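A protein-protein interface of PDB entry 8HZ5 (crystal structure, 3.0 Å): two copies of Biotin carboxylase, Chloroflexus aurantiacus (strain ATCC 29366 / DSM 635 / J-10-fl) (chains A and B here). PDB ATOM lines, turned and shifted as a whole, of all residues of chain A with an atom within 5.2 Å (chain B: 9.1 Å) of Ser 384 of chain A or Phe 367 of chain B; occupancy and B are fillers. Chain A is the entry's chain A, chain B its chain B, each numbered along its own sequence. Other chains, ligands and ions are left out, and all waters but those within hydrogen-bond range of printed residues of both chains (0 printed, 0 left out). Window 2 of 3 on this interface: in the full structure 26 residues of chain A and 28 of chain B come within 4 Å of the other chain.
OG of Ser 384 of chain A sits at hydrogen-bond distance from OG of Ser 384 of chain B (3.5 Å).
N of Leu 369 of chain B sits at hydrogen-bond distance from O of Val 421 of chain B (3.2 Å).
The backbone NH (N) of Tyr 368 of chain B sits at hydrogen-bond distance from the side-chain hydroxyl (OG) of Ser 384 of chain B, at 3.1 Å.
The backbone NH of Tyr 368 of chain A is in hydrogen-bond range of the side-chain hydroxyl of Ser 384 of chain A.
N of Thr 423 of chain B lies within hydrogen-bond range of O of Phe 367 of chain B (3.0 Å).
Among the printed residues, merely in contact across the chains: Ser 384 of chain A with Phe 367 of chain B, Phe 367 of chain A with Ser 384 of chain B, Phe 367 of chain A with Tyr 383 of chain B, Leu 382 of chain A with Leu 369 of chain B, Tyr 383 of chain A with Phe 367 of chain B, Arg 53 of chain A with Phe 367 of chain B, Tyr 383 of chain A with Leu 369 of chain B and Arg 53 of chain A with Val 421 of chain B.
Of chain B, only Phe 367 and Ser 384 come within 4 Å of Ser 384 of chain A.
Phe 367 of chain B touches just these residues of chain A: Arg 53 (3.9 Å), Tyr 383 (3.8 Å) and Ser 384 (3.4 Å).
Gly 385 of chain A touches none of the printed residues of chain B.
Of the printed residues of chain B, Phe 367 of chain A touches Tyr 383 (3.7 Å) and Ser 384 (3.5 Å).
Printed residues of chain B within 4 Å of Arg 53 of chain A: Phe 367 (3.9 Å) and Val 421 (3.9 Å).
Of the printed residues of chain B, Leu 382 of chain A touches Leu 369 (3.7 Å).
Of the printed residues of chain A, Val 421 of chain B touches Arg 53 (3.9 Å).
Tyr 386 of chain A touches none of the printed residues of chain B.
The nearest residue of chain B that does not touch Ser 384 of chain A is Tyr 368 of chain B (4.4 Å).
The nearest printed residue of chain A that does not touch Phe 367 of chain B is Gly 385 of chain A (5.4 Å).
Printed residues of chain A that touch a printed residue of chain B: Arg 53, Phe 367, Leu 382, Tyr 383 and Ser 384.
Hydrophobic or aromatic side chains of chain A that line the printed part of chain B: Phe 367 and Tyr 383.
Phe 367 of chain A touches Tyr 383 of chain B, and with the chains exchanged Tyr 383 of chain A touches Phe 367 of chain B.
Phe 367 of chain A touches Ser 384 of chain B, and with the chains exchanged Ser 384 of chain A touches Phe 367 of chain B.
Ser 384 of chain A touches its own counterpart, Ser 384 of chain B.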
ATOM      1  N   ARG A  53      -4.629  -5.961  -9.151  1.00  0.00           N
ATOM      2  CA  ARG A  53      -5.612  -6.080  -8.093  1.00  0.00           C
ATOM      3  C   ARG A  53      -6.327  -4.810  -7.774  1.00  0.00           C
ATOM      4  O   ARG A  53      -7.540  -4.793  -7.669  1.00  0.00           O
ATOM      5  CB  ARG A  53      -4.869  -6.526  -6.848  1.00  0.00           C
ATOM      6  CG  ARG A  53      -5.700  -6.926  -5.646  1.00  0.00           C
ATOM      7  CD  ARG A  53      -4.795  -7.073  -4.437  1.00  0.00           C
ATOM      8  NE  ARG A  53      -5.123  -8.237  -3.620  1.00  0.00           N
ATOM      9  CZ  ARG A  53      -4.227  -8.942  -2.938  1.00  0.00           C
ATOM     10  NH1 ARG A  53      -2.944  -8.616  -2.987  1.00  0.00           N
ATOM     11  NH2 ARG A  53      -4.613  -9.987  -2.219  1.00  0.00           N
ATOM     12  N   VAL A 365       9.838 -10.958  -2.250  1.00  0.00           N
ATOM     13  CA  VAL A 365       9.656 -10.161  -1.073  1.00  0.00           C
ATOM     14  C   VAL A 365       8.770 -11.077  -0.323  1.00  0.00           C
ATOM     15  O   VAL A 365       7.571 -11.028  -0.462  1.00  0.00           O
ATOM     16  CB  VAL A 365       8.925  -8.858  -1.367  1.00  0.00           C
ATOM     17  CG1 VAL A 365       8.808  -8.006  -0.120  1.00  0.00           C
ATOM     18  CG2 VAL A 365       9.639  -8.095  -2.468  1.00  0.00           C
ATOM     19  N   GLU A 366       9.372 -11.959   0.448  1.00  0.00           N
ATOM     20  CA  GLU A 366       8.642 -12.918   1.241  1.00  0.00           C
ATOM     21  C   GLU A 366       7.854 -12.222   2.287  1.00  0.00           C
ATOM     22  O   GLU A 366       6.744 -12.617   2.592  1.00  0.00           O
ATOM     23  CB  GLU A 366       9.645 -13.863   1.872  1.00  0.00           C
ATOM     24  CG  GLU A 366      10.678 -14.389   0.900  1.00  0.00           C
ATOM     25  CD  GLU A 366      11.713 -15.255   1.576  1.00  0.00           C
ATOM     26  OE1 GLU A 366      11.457 -15.713   2.703  1.00  0.00           O
ATOM     27  OE2 GLU A 366      12.778 -15.479   0.975  1.00  0.00           O
ATOM     28  N   PHE A 367       8.446 -11.201   2.874  1.00  0.00           N
ATOM     29  CA  PHE A 367       7.765 -10.417   3.857  1.00  0.00           C
ATOM     30  C   PHE A 367       7.928  -8.972   3.544  1.00  0.00           C
ATOM     31  O   PHE A 367       9.011  -8.537   3.230  1.00  0.00           O
ATOM     32  CB  PHE A 367       8.334 -10.721   5.236  1.00  0.00           C
ATOM     33  CG  PHE A 367       7.654 -10.001   6.353  1.00  0.00           C
ATOM     34  CD1 PHE A 367       6.477 -10.467   6.874  1.00  0.00           C
ATOM     35  CD2 PHE A 367       8.216  -8.873   6.894  1.00  0.00           C
ATOM     36  CE1 PHE A 367       5.859  -9.803   7.901  1.00  0.00           C
ATOM     37  CE2 PHE A 367       7.604  -8.203   7.921  1.00  0.00           C
ATOM     38  CZ  PHE A 367       6.425  -8.669   8.424  1.00  0.00           C
ATOM     39  N   TYR A 368       6.836  -8.226   3.601  1.00  0.00           N
ATOM     40  CA  TYR A 368       6.890  -6.800   3.420  1.00  0.00           C
ATOM     41  C   TYR A 368       6.102  -6.153   4.486  1.00  0.00           C
ATOM     42  O   TYR A 368       4.898  -6.331   4.566  1.00  0.00           O
ATOM     43  CB  TYR A 368       6.340  -6.371   2.079  1.00  0.00           C
ATOM     44  CG  TYR A 368       6.299  -4.893   1.842  1.00  0.00           C
ATOM     45  CD1 TYR A 368       7.409  -4.104   2.051  1.00  0.00           C
ATOM     46  CD2 TYR A 368       5.146  -4.291   1.397  1.00  0.00           C
ATOM     47  CE1 TYR A 368       7.364  -2.748   1.834  1.00  0.00           C
ATOM     48  CE2 TYR A 368       5.097  -2.942   1.162  1.00  0.00           C
ATOM     49  CZ  TYR A 368       6.209  -2.178   1.388  1.00  0.00           C
ATOM     50  OH  TYR A 368       6.154  -0.835   1.166  1.00  0.00           O
ATOM     51  N   LEU A 382       4.736  -3.046  -3.547  1.00  0.00           N
ATOM     52  CA  LEU A 382       5.167  -4.280  -2.978  1.00  0.00           C
ATOM     53  C   LEU A 382       4.174  -4.914  -2.079  1.00  0.00           C
ATOM     54  O   LEU A 382       3.299  -4.253  -1.550  1.00  0.00           O
ATOM     55  CB  LEU A 382       6.466  -4.107  -2.212  1.00  0.00           C
ATOM     56  CG  LEU A 382       7.818  -3.758  -2.804  1.00  0.00           C
ATOM     57  CD1 LEU A 382       8.874  -4.080  -1.776  1.00  0.00           C
ATOM     58  CD2 LEU A 382       8.093  -4.488  -4.094  1.00  0.00           C
ATOM     59  N   TYR A 383       4.318  -6.216  -1.913  1.00  0.00           N
ATOM     60  CA  TYR A 383       3.454  -6.961  -1.055  1.00  0.00           C
ATOM     61  C   TYR A 383       4.245  -8.185  -0.703  1.00  0.00           C
ATOM     62  O   TYR A 383       5.240  -8.480  -1.339  1.00  0.00           O
ATOM     63  CB  TYR A 383       2.135  -7.335  -1.731  1.00  0.00           C
ATOM     64  CG  TYR A 383       2.204  -8.163  -2.981  1.00  0.00           C
ATOM     65  CD1 TYR A 383       2.310  -7.566  -4.222  1.00  0.00           C
ATOM     66  CD2 TYR A 383       2.105  -9.538  -2.924  1.00  0.00           C
ATOM     67  CE1 TYR A 383       2.356  -8.324  -5.363  1.00  0.00           C
ATOM     68  CE2 TYR A 383       2.156 -10.300  -4.060  1.00  0.00           C
ATOM     69  CZ  TYR A 383       2.282  -9.689  -5.274  1.00  0.00           C
ATOM     70  OH  TYR A 383       2.331 -10.465  -6.399  1.00  0.00           O
ATOM     71  N   SER A 384       3.819  -8.889   0.332  1.00  0.00           N
ATOM     72  CA  SER A 384       4.489 -10.097   0.733  1.00  0.00           C
ATOM     73  C   SER A 384       4.087 -11.220  -0.174  1.00  0.00           C
ATOM     74  O   SER A 384       2.946 -11.614  -0.192  1.00  0.00           O
ATOM     75  CB  SER A 384       4.136 -10.429   2.163  1.00  0.00           C
ATOM     76  OG  SER A 384       4.163  -9.277   2.975  1.00  0.00           O
ATOM     77  N   GLY A 385       5.029 -11.737  -0.939  1.00  0.00           N
ATOM     78  CA  GLY A 385       4.747 -12.821  -1.839  1.00  0.00           C
ATOM     79  C   GLY A 385       5.023 -12.360  -3.223  1.00  0.00           C
ATOM     80  O   GLY A 385       4.617 -13.003  -4.171  1.00  0.00           O
ATOM     81  N   TYR A 386       5.728 -11.255  -3.346  1.00  0.00           N
ATOM     82  CA  TYR A 386       5.994 -10.677  -4.627  1.00  0.00           C
ATOM     83  C   TYR A 386       7.296 -11.069  -5.162  1.00  0.00           C
ATOM     84  O   TYR A 386       8.288 -10.837  -4.535  1.00  0.00           O
ATOM     85  CB  TYR A 386       6.007  -9.172  -4.485  1.00  0.00           C
ATOM     86  CG  TYR A 386       6.074  -8.377  -5.763  1.00  0.00           C
ATOM     87  CD1 TYR A 386       5.424  -8.786  -6.913  1.00  0.00           C
ATOM     88  CD2 TYR A 386       6.775  -7.198  -5.807  1.00  0.00           C
ATOM     89  CE1 TYR A 386       5.485  -8.040  -8.069  1.00  0.00           C
ATOM     90  CE2 TYR A 386       6.848  -6.450  -6.953  1.00  0.00           C
ATOM     91  CZ  TYR A 386       6.194  -6.872  -8.078  1.00  0.00           C
ATOM     92  OH  TYR A 386       6.266  -6.115  -9.218  1.00  0.00           O
ATOM     93  N   GLU B 364      -4.214 -16.392  12.834  1.00  0.00           N
ATOM     94  CA  GLU B 364      -3.088 -15.884  12.084  1.00  0.00           C
ATOM     95  C   GLU B 364      -3.472 -14.966  10.946  1.00  0.00           C
ATOM     96  O   GLU B 364      -4.326 -15.293  10.140  1.00  0.00           O
ATOM     97  CB  GLU B 364      -2.159 -17.006  11.619  1.00  0.00           C
ATOM     98  CG  GLU B 364      -2.754 -18.029  10.660  1.00  0.00           C
ATOM     99  CD  GLU B 364      -3.543 -19.131  11.347  1.00  0.00           C
ATOM    100  OE1 GLU B 364      -3.076 -19.659  12.379  1.00  0.00           O
ATOM    101  OE2 GLU B 364      -4.640 -19.466  10.850  1.00  0.00           O
ATOM    102  N   VAL B 365      -2.877 -13.783  10.899  1.00  0.00           N
ATOM    103  CA  VAL B 365      -3.113 -12.890   9.798  1.00  0.00           C
ATOM    104  C   VAL B 365      -2.127 -13.403   8.823  1.00  0.00           C
ATOM    105  O   VAL B 365      -0.961 -13.183   8.974  1.00  0.00           O
ATOM    106  CB  VAL B 365      -2.759 -11.435  10.148  1.00  0.00           C
ATOM    107  CG1 VAL B 365      -3.127 -10.503   9.011  1.00  0.00           C
ATOM    108  CG2 VAL B 365      -3.443 -10.994  11.425  1.00  0.00           C
ATOM    109  N   GLU B 366      -2.587 -14.108   7.817  1.00  0.00           N
ATOM    110  CA  GLU B 366      -1.673 -14.729   6.887  1.00  0.00           C
ATOM    111  C   GLU B 366      -1.125 -13.750   5.910  1.00  0.00           C
ATOM    112  O   GLU B 366      -0.005 -13.892   5.449  1.00  0.00           O
ATOM    113  CB  GLU B 366      -2.365 -15.867   6.146  1.00  0.00           C
ATOM    114  CG  GLU B 366      -3.472 -16.572   6.898  1.00  0.00           C
ATOM    115  CD  GLU B 366      -4.363 -17.367   5.967  1.00  0.00           C
ATOM    116  OE1 GLU B 366      -4.161 -17.276   4.739  1.00  0.00           O
ATOM    117  OE2 GLU B 366      -5.261 -18.080   6.455  1.00  0.00           O
ATOM    118  N   PHE B 367      -1.921 -12.758   5.576  1.00  0.00           N
ATOM    119  CA  PHE B 367      -1.453 -11.722   4.710  1.00  0.00           C
ATOM    120  C   PHE B 367      -1.902 -10.390   5.203  1.00  0.00           C
ATOM    121  O   PHE B 367      -3.072 -10.145   5.322  1.00  0.00           O
ATOM    122  CB  PHE B 367      -1.910 -11.935   3.288  1.00  0.00           C
ATOM    123  CG  PHE B 367      -1.366 -10.931   2.317  1.00  0.00           C
ATOM    124  CD1 PHE B 367      -0.009 -10.782   2.146  1.00  0.00           C
ATOM    125  CD2 PHE B 367      -2.217 -10.141   1.574  1.00  0.00           C
ATOM    126  CE1 PHE B 367       0.486  -9.856   1.259  1.00  0.00           C
ATOM    127  CE2 PHE B 367      -1.726  -9.217   0.682  1.00  0.00           C
ATOM    128  CZ  PHE B 367      -0.370  -9.077   0.525  1.00  0.00           C
ATOM    129  N   TYR B 368      -0.954  -9.540   5.514  1.00  0.00           N
ATOM    130  CA  TYR B 368      -1.264  -8.169   5.904  1.00  0.00           C
ATOM    131  C   TYR B 368      -0.611  -7.197   4.918  1.00  0.00           C
ATOM    132  O   TYR B 368       0.600  -7.268   4.669  1.00  0.00           O
ATOM    133  CB  TYR B 368      -0.808  -7.868   7.324  1.00  0.00           C
ATOM    134  CG  TYR B 368      -0.957  -6.397   7.693  1.00  0.00           C
ATOM    135  CD1 TYR B 368      -2.204  -5.774   7.665  1.00  0.00           C
ATOM    136  CD2 TYR B 368       0.150  -5.628   8.051  1.00  0.00           C
ATOM    137  CE1 TYR B 368      -2.339  -4.425   7.994  1.00  0.00           C
ATOM    138  CE2 TYR B 368       0.019  -4.297   8.378  1.00  0.00           C
ATOM    139  CZ  TYR B 368      -1.226  -3.696   8.347  1.00  0.00           C
ATOM    140  OH  TYR B 368      -1.366  -2.364   8.675  1.00  0.00           O
ATOM    141  N   LEU B 369      -1.429  -6.283   4.371  1.00  0.00           N
ATOM    142  CA  LEU B 369      -1.002  -5.252   3.437  1.00  0.00           C
ATOM    143  C   LEU B 369      -1.698  -3.928   3.730  1.00  0.00           C
ATOM    144  O   LEU B 369      -2.897  -3.749   3.436  1.00  0.00           O
ATOM    145  CB  LEU B 369      -1.275  -5.686   1.999  1.00  0.00           C
ATOM    146  CG  LEU B 369      -0.736  -4.744   0.934  1.00  0.00           C
ATOM    147  CD1 LEU B 369       0.754  -4.465   1.155  1.00  0.00           C
ATOM    148  CD2 LEU B 369      -0.992  -5.374  -0.412  1.00  0.00           C
ATOM    149  N   PRO B 370      -0.936  -3.000   4.373  1.00  0.00           N
ATOM    150  CA  PRO B 370      -1.655  -1.787   4.691  1.00  0.00           C
ATOM    151  C   PRO B 370      -1.837  -0.864   3.544  1.00  0.00           C
ATOM    152  O   PRO B 370      -1.112  -0.906   2.564  1.00  0.00           O
ATOM    153  CB  PRO B 370      -0.751  -1.123   5.704  1.00  0.00           C
ATOM    154  CG  PRO B 370       0.594  -1.528   5.362  1.00  0.00           C
ATOM    155  CD  PRO B 370       0.428  -2.945   4.979  1.00  0.00           C
ATOM    156  N   LEU B 382      -0.102  -5.185  13.029  1.00  0.00           N
ATOM    157  CA  LEU B 382      -0.296  -6.345  12.220  1.00  0.00           C
ATOM    158  C   LEU B 382       0.892  -6.630  11.356  1.00  0.00           C
ATOM    159  O   LEU B 382       1.661  -5.733  11.056  1.00  0.00           O
ATOM    160  CB  LEU B 382      -1.579  -6.292  11.386  1.00  0.00           C
ATOM    161  CG  LEU B 382      -2.897  -6.412  12.088  1.00  0.00           C
ATOM    162  CD1 LEU B 382      -3.845  -7.012  11.072  1.00  0.00           C
ATOM    163  CD2 LEU B 382      -2.668  -7.321  13.274  1.00  0.00           C
ATOM    164  N   TYR B 383       1.070  -7.890  10.992  1.00  0.00           N
ATOM    165  CA  TYR B 383       2.118  -8.286  10.078  1.00  0.00           C
ATOM    166  C   TYR B 383       1.620  -9.580   9.477  1.00  0.00           C
ATOM    167  O   TYR B 383       0.688 -10.173   9.980  1.00  0.00           O
ATOM    168  CB  TYR B 383       3.534  -8.355  10.685  1.00  0.00           C
ATOM    169  CG  TYR B 383       3.827  -9.384  11.718  1.00  0.00           C
ATOM    170  CD1 TYR B 383       4.212 -10.656  11.357  1.00  0.00           C
ATOM    171  CD2 TYR B 383       3.801  -9.062  13.058  1.00  0.00           C
ATOM    172  CE1 TYR B 383       4.507 -11.602  12.301  1.00  0.00           C
ATOM    173  CE2 TYR B 383       4.097 -10.002  14.009  1.00  0.00           C
ATOM    174  CZ  TYR B 383       4.431 -11.276  13.621  1.00  0.00           C
ATOM    175  OH  TYR B 383       4.722 -12.230  14.557  1.00  0.00           O
ATOM    176  N   SER B 384       2.186  -9.975   8.353  1.00  0.00           N
ATOM    177  CA  SER B 384       1.792 -11.195   7.695  1.00  0.00           C
ATOM    178  C   SER B 384       2.444 -12.286   8.469  1.00  0.00           C
ATOM    179  O   SER B 384       3.653 -12.403   8.462  1.00  0.00           O
ATOM    180  CB  SER B 384       2.241 -11.141   6.248  1.00  0.00           C
ATOM    181  OG  SER B 384       2.163  -9.825   5.738  1.00  0.00           O
ATOM    182  N   GLY B 385       1.650 -13.116   9.118  1.00  0.00           N
ATOM    183  CA  GLY B 385       2.210 -14.105  10.029  1.00  0.00           C
ATOM    184  C   GLY B 385       1.871 -13.863  11.486  1.00  0.00           C
ATOM    185  O   GLY B 385       2.044 -14.770  12.320  1.00  0.00           O
ATOM    186  N   TYR B 386       1.394 -12.669  11.826  1.00  0.00           N
ATOM    187  CA  TYR B 386       1.070 -12.354  13.206  1.00  0.00           C
ATOM    188  C   TYR B 386      -0.139 -13.157  13.665  1.00  0.00           C
ATOM    189  O   TYR B 386      -1.168 -13.182  12.986  1.00  0.00           O
ATOM    190  CB  TYR B 386       0.796 -10.861  13.347  1.00  0.00           C
ATOM    191  CG  TYR B 386       0.392 -10.460  14.746  1.00  0.00           C
ATOM    192  CD1 TYR B 386       1.286 -10.566  15.798  1.00  0.00           C
ATOM    193  CD2 TYR B 386      -0.865  -9.948  15.004  1.00  0.00           C
ATOM    194  CE1 TYR B 386       0.949 -10.195  17.063  1.00  0.00           C
ATOM    195  CE2 TYR B 386      -1.222  -9.578  16.282  1.00  0.00           C
ATOM    196  CZ  TYR B 386      -0.307  -9.700  17.319  1.00  0.00           C
ATOM    197  OH  TYR B 386      -0.655  -9.313  18.612  1.00  0.00           O
ATOM    198  N   GLU B 419      -8.109  -1.299   0.055  1.00  0.00           N
ATOM    199  CA  GLU B 419      -6.735  -1.692  -0.146  1.00  0.00           C
ATOM    200  C   GLU B 419      -6.186  -2.514   1.010  1.00  0.00           C
ATOM    201  O   GLU B 419      -5.231  -3.232   0.839  1.00  0.00           O
ATOM    202  CB  GLU B 419      -5.868  -0.453  -0.333  1.00  0.00           C
ATOM    203  CG  GLU B 419      -6.008   0.248  -1.656  1.00  0.00           C
ATOM    204  CD  GLU B 419      -5.016   1.367  -1.804  1.00  0.00           C
ATOM    205  OE1 GLU B 419      -4.236   1.595  -0.870  1.00  0.00           O
ATOM    206  OE2 GLU B 419      -5.018   2.016  -2.858  1.00  0.00           O
ATOM    207  N   CYS B 420      -6.761  -2.405   2.185  1.00  0.00           N
ATOM    208  CA  CYS B 420      -6.243  -3.146   3.296  1.00  0.00           C
ATOM    209  C   CYS B 420      -6.593  -4.577   3.137  1.00  0.00           C
ATOM    210  O   CYS B 420      -7.755  -4.920   3.014  1.00  0.00           O
ATOM    211  CB  CYS B 420      -6.772  -2.641   4.637  1.00  0.00           C
ATOM    212  SG  CYS B 420      -5.704  -2.906   6.058  1.00  0.00           S
ATOM    213  N   VAL B 421      -5.577  -5.427   3.048  1.00  0.00           N
ATOM    214  CA  VAL B 421      -5.824  -6.855   2.945  1.00  0.00           C
ATOM    215  C   VAL B 421      -5.420  -7.503   4.240  1.00  0.00           C
ATOM    216  O   VAL B 421      -4.240  -7.702   4.478  1.00  0.00           O
ATOM    217  CB  VAL B 421      -5.049  -7.523   1.792  1.00  0.00           C
ATOM    218  CG1 VAL B 421      -5.769  -8.784   1.345  1.00  0.00           C
ATOM    219  CG2 VAL B 421      -4.882  -6.575   0.616  1.00  0.00           C
ATOM    220  N   ILE B 422      -6.386  -7.782   5.104  1.00  0.00           N
ATOM    221  CA  ILE B 422      -6.089  -8.499   6.333  1.00  0.00           C
ATOM    222  C   ILE B 422      -6.718  -9.855   6.119  1.00  0.00           C
ATOM    223  O   ILE B 422      -7.938 -10.005   6.214  1.00  0.00           O
ATOM    224  CB  ILE B 422      -6.681  -7.807   7.569  1.00  0.00           C
ATOM    225  CG1 ILE B 422      -6.121  -6.391   7.698  1.00  0.00           C
ATOM    226  CG2 ILE B 422      -6.382  -8.611   8.825  1.00  0.00           C
ATOM    227  CD1 ILE B 422      -6.659  -5.620   8.881  1.00  0.00           C
ATOM    228  N   THR B 423      -5.903 -10.849   5.798  1.00  0.00           N
ATOM    229  CA  THR B 423      -6.457 -12.154   5.472  1.00  0.00           C
ATOM    230  C   THR B 423      -6.229 -13.200   6.541  1.00  0.00           C
ATOM    231  O   THR B 423      -5.194 -13.198   7.192  1.00  0.00           O
ATOM    232  CB  THR B 423      -5.873 -12.667   4.145  1.00  0.00           C
ATOM    233  OG1 THR B 423      -5.238 -11.583   3.460  1.00  0.00           O
ATOM    234  CG2 THR B 423      -6.973 -13.229   3.263  1.00  0.00           C
ATOM    235  N   GLY B 424      -7.199 -14.089   6.730  1.00  0.00           N
ATOM    236  CA  GLY B 424      -7.046 -15.161   7.678  1.00  0.00           C
ATOM    237  C   GLY B 424      -7.832 -14.910   8.910  1.00  0.00           C
ATOM    238  O   GLY B 424      -8.127 -15.835   9.646  1.00  0.00           O
ATOM    239  N   ILE B 425      -8.147 -13.654   9.169  1.00  0.00           N
ATOM    240  CA  ILE B 425      -8.952 -13.297  10.307  1.00  0.00           C
ATOM    241  C   ILE B 425      -9.993 -12.451   9.658  1.00  0.00           C
ATOM    242  O   ILE B 425      -9.720 -11.796   8.677  1.00  0.00           O
ATOM    243  CB  ILE B 425      -8.173 -12.451  11.316  1.00  0.00           C
ATOM    244  CG1 ILE B 425      -6.813 -13.056  11.610  1.00  0.00           C
ATOM    245  CG2 ILE B 425      -8.905 -12.356  12.643  1.00  0.00           C
ATOM    246  CD1 ILE B 425      -6.877 -14.093  12.706  1.00  0.00           C
ATOM    247  N   THR B 427     -12.594  -9.227   9.793  1.00  0.00           N
ATOM    248  CA  THR B 427     -12.368  -7.923  10.342  1.00  0.00           C
ATOM    249  C   THR B 427     -13.601  -7.098  10.286  1.00  0.00           C
ATOM    250  O   THR B 427     -14.640  -7.588   9.889  1.00  0.00           O
ATOM    251  CB  THR B 427     -11.301  -7.243   9.474  1.00  0.00           C
ATOM    252  OG1 THR B 427     -11.635  -7.405   8.093  1.00  0.00           O
ATOM    253  CG2 THR B 427      -9.951  -7.839   9.710  1.00  0.00           C
ATOM    254  N   ILE B 429     -13.574  -4.152   8.531  1.00  0.00           N
ATOM    255  CA  ILE B 429     -13.480  -3.351   7.322  1.00  0.00           C
ATOM    256  C   ILE B 429     -14.731  -3.256   6.458  1.00  0.00           C
ATOM    257  O   ILE B 429     -15.088  -2.172   6.040  1.00  0.00           O
ATOM    258  CB  ILE B 429     -12.305  -3.784   6.418  1.00  0.00           C
ATOM    259  CG1 ILE B 429     -11.103  -4.236   7.213  1.00  0.00           C
ATOM    260  CG2 ILE B 429     -11.898  -2.678   5.476  1.00  0.00           C
ATOM    261  CD1 ILE B 429      -9.914  -4.558   6.339  1.00  0.00           C
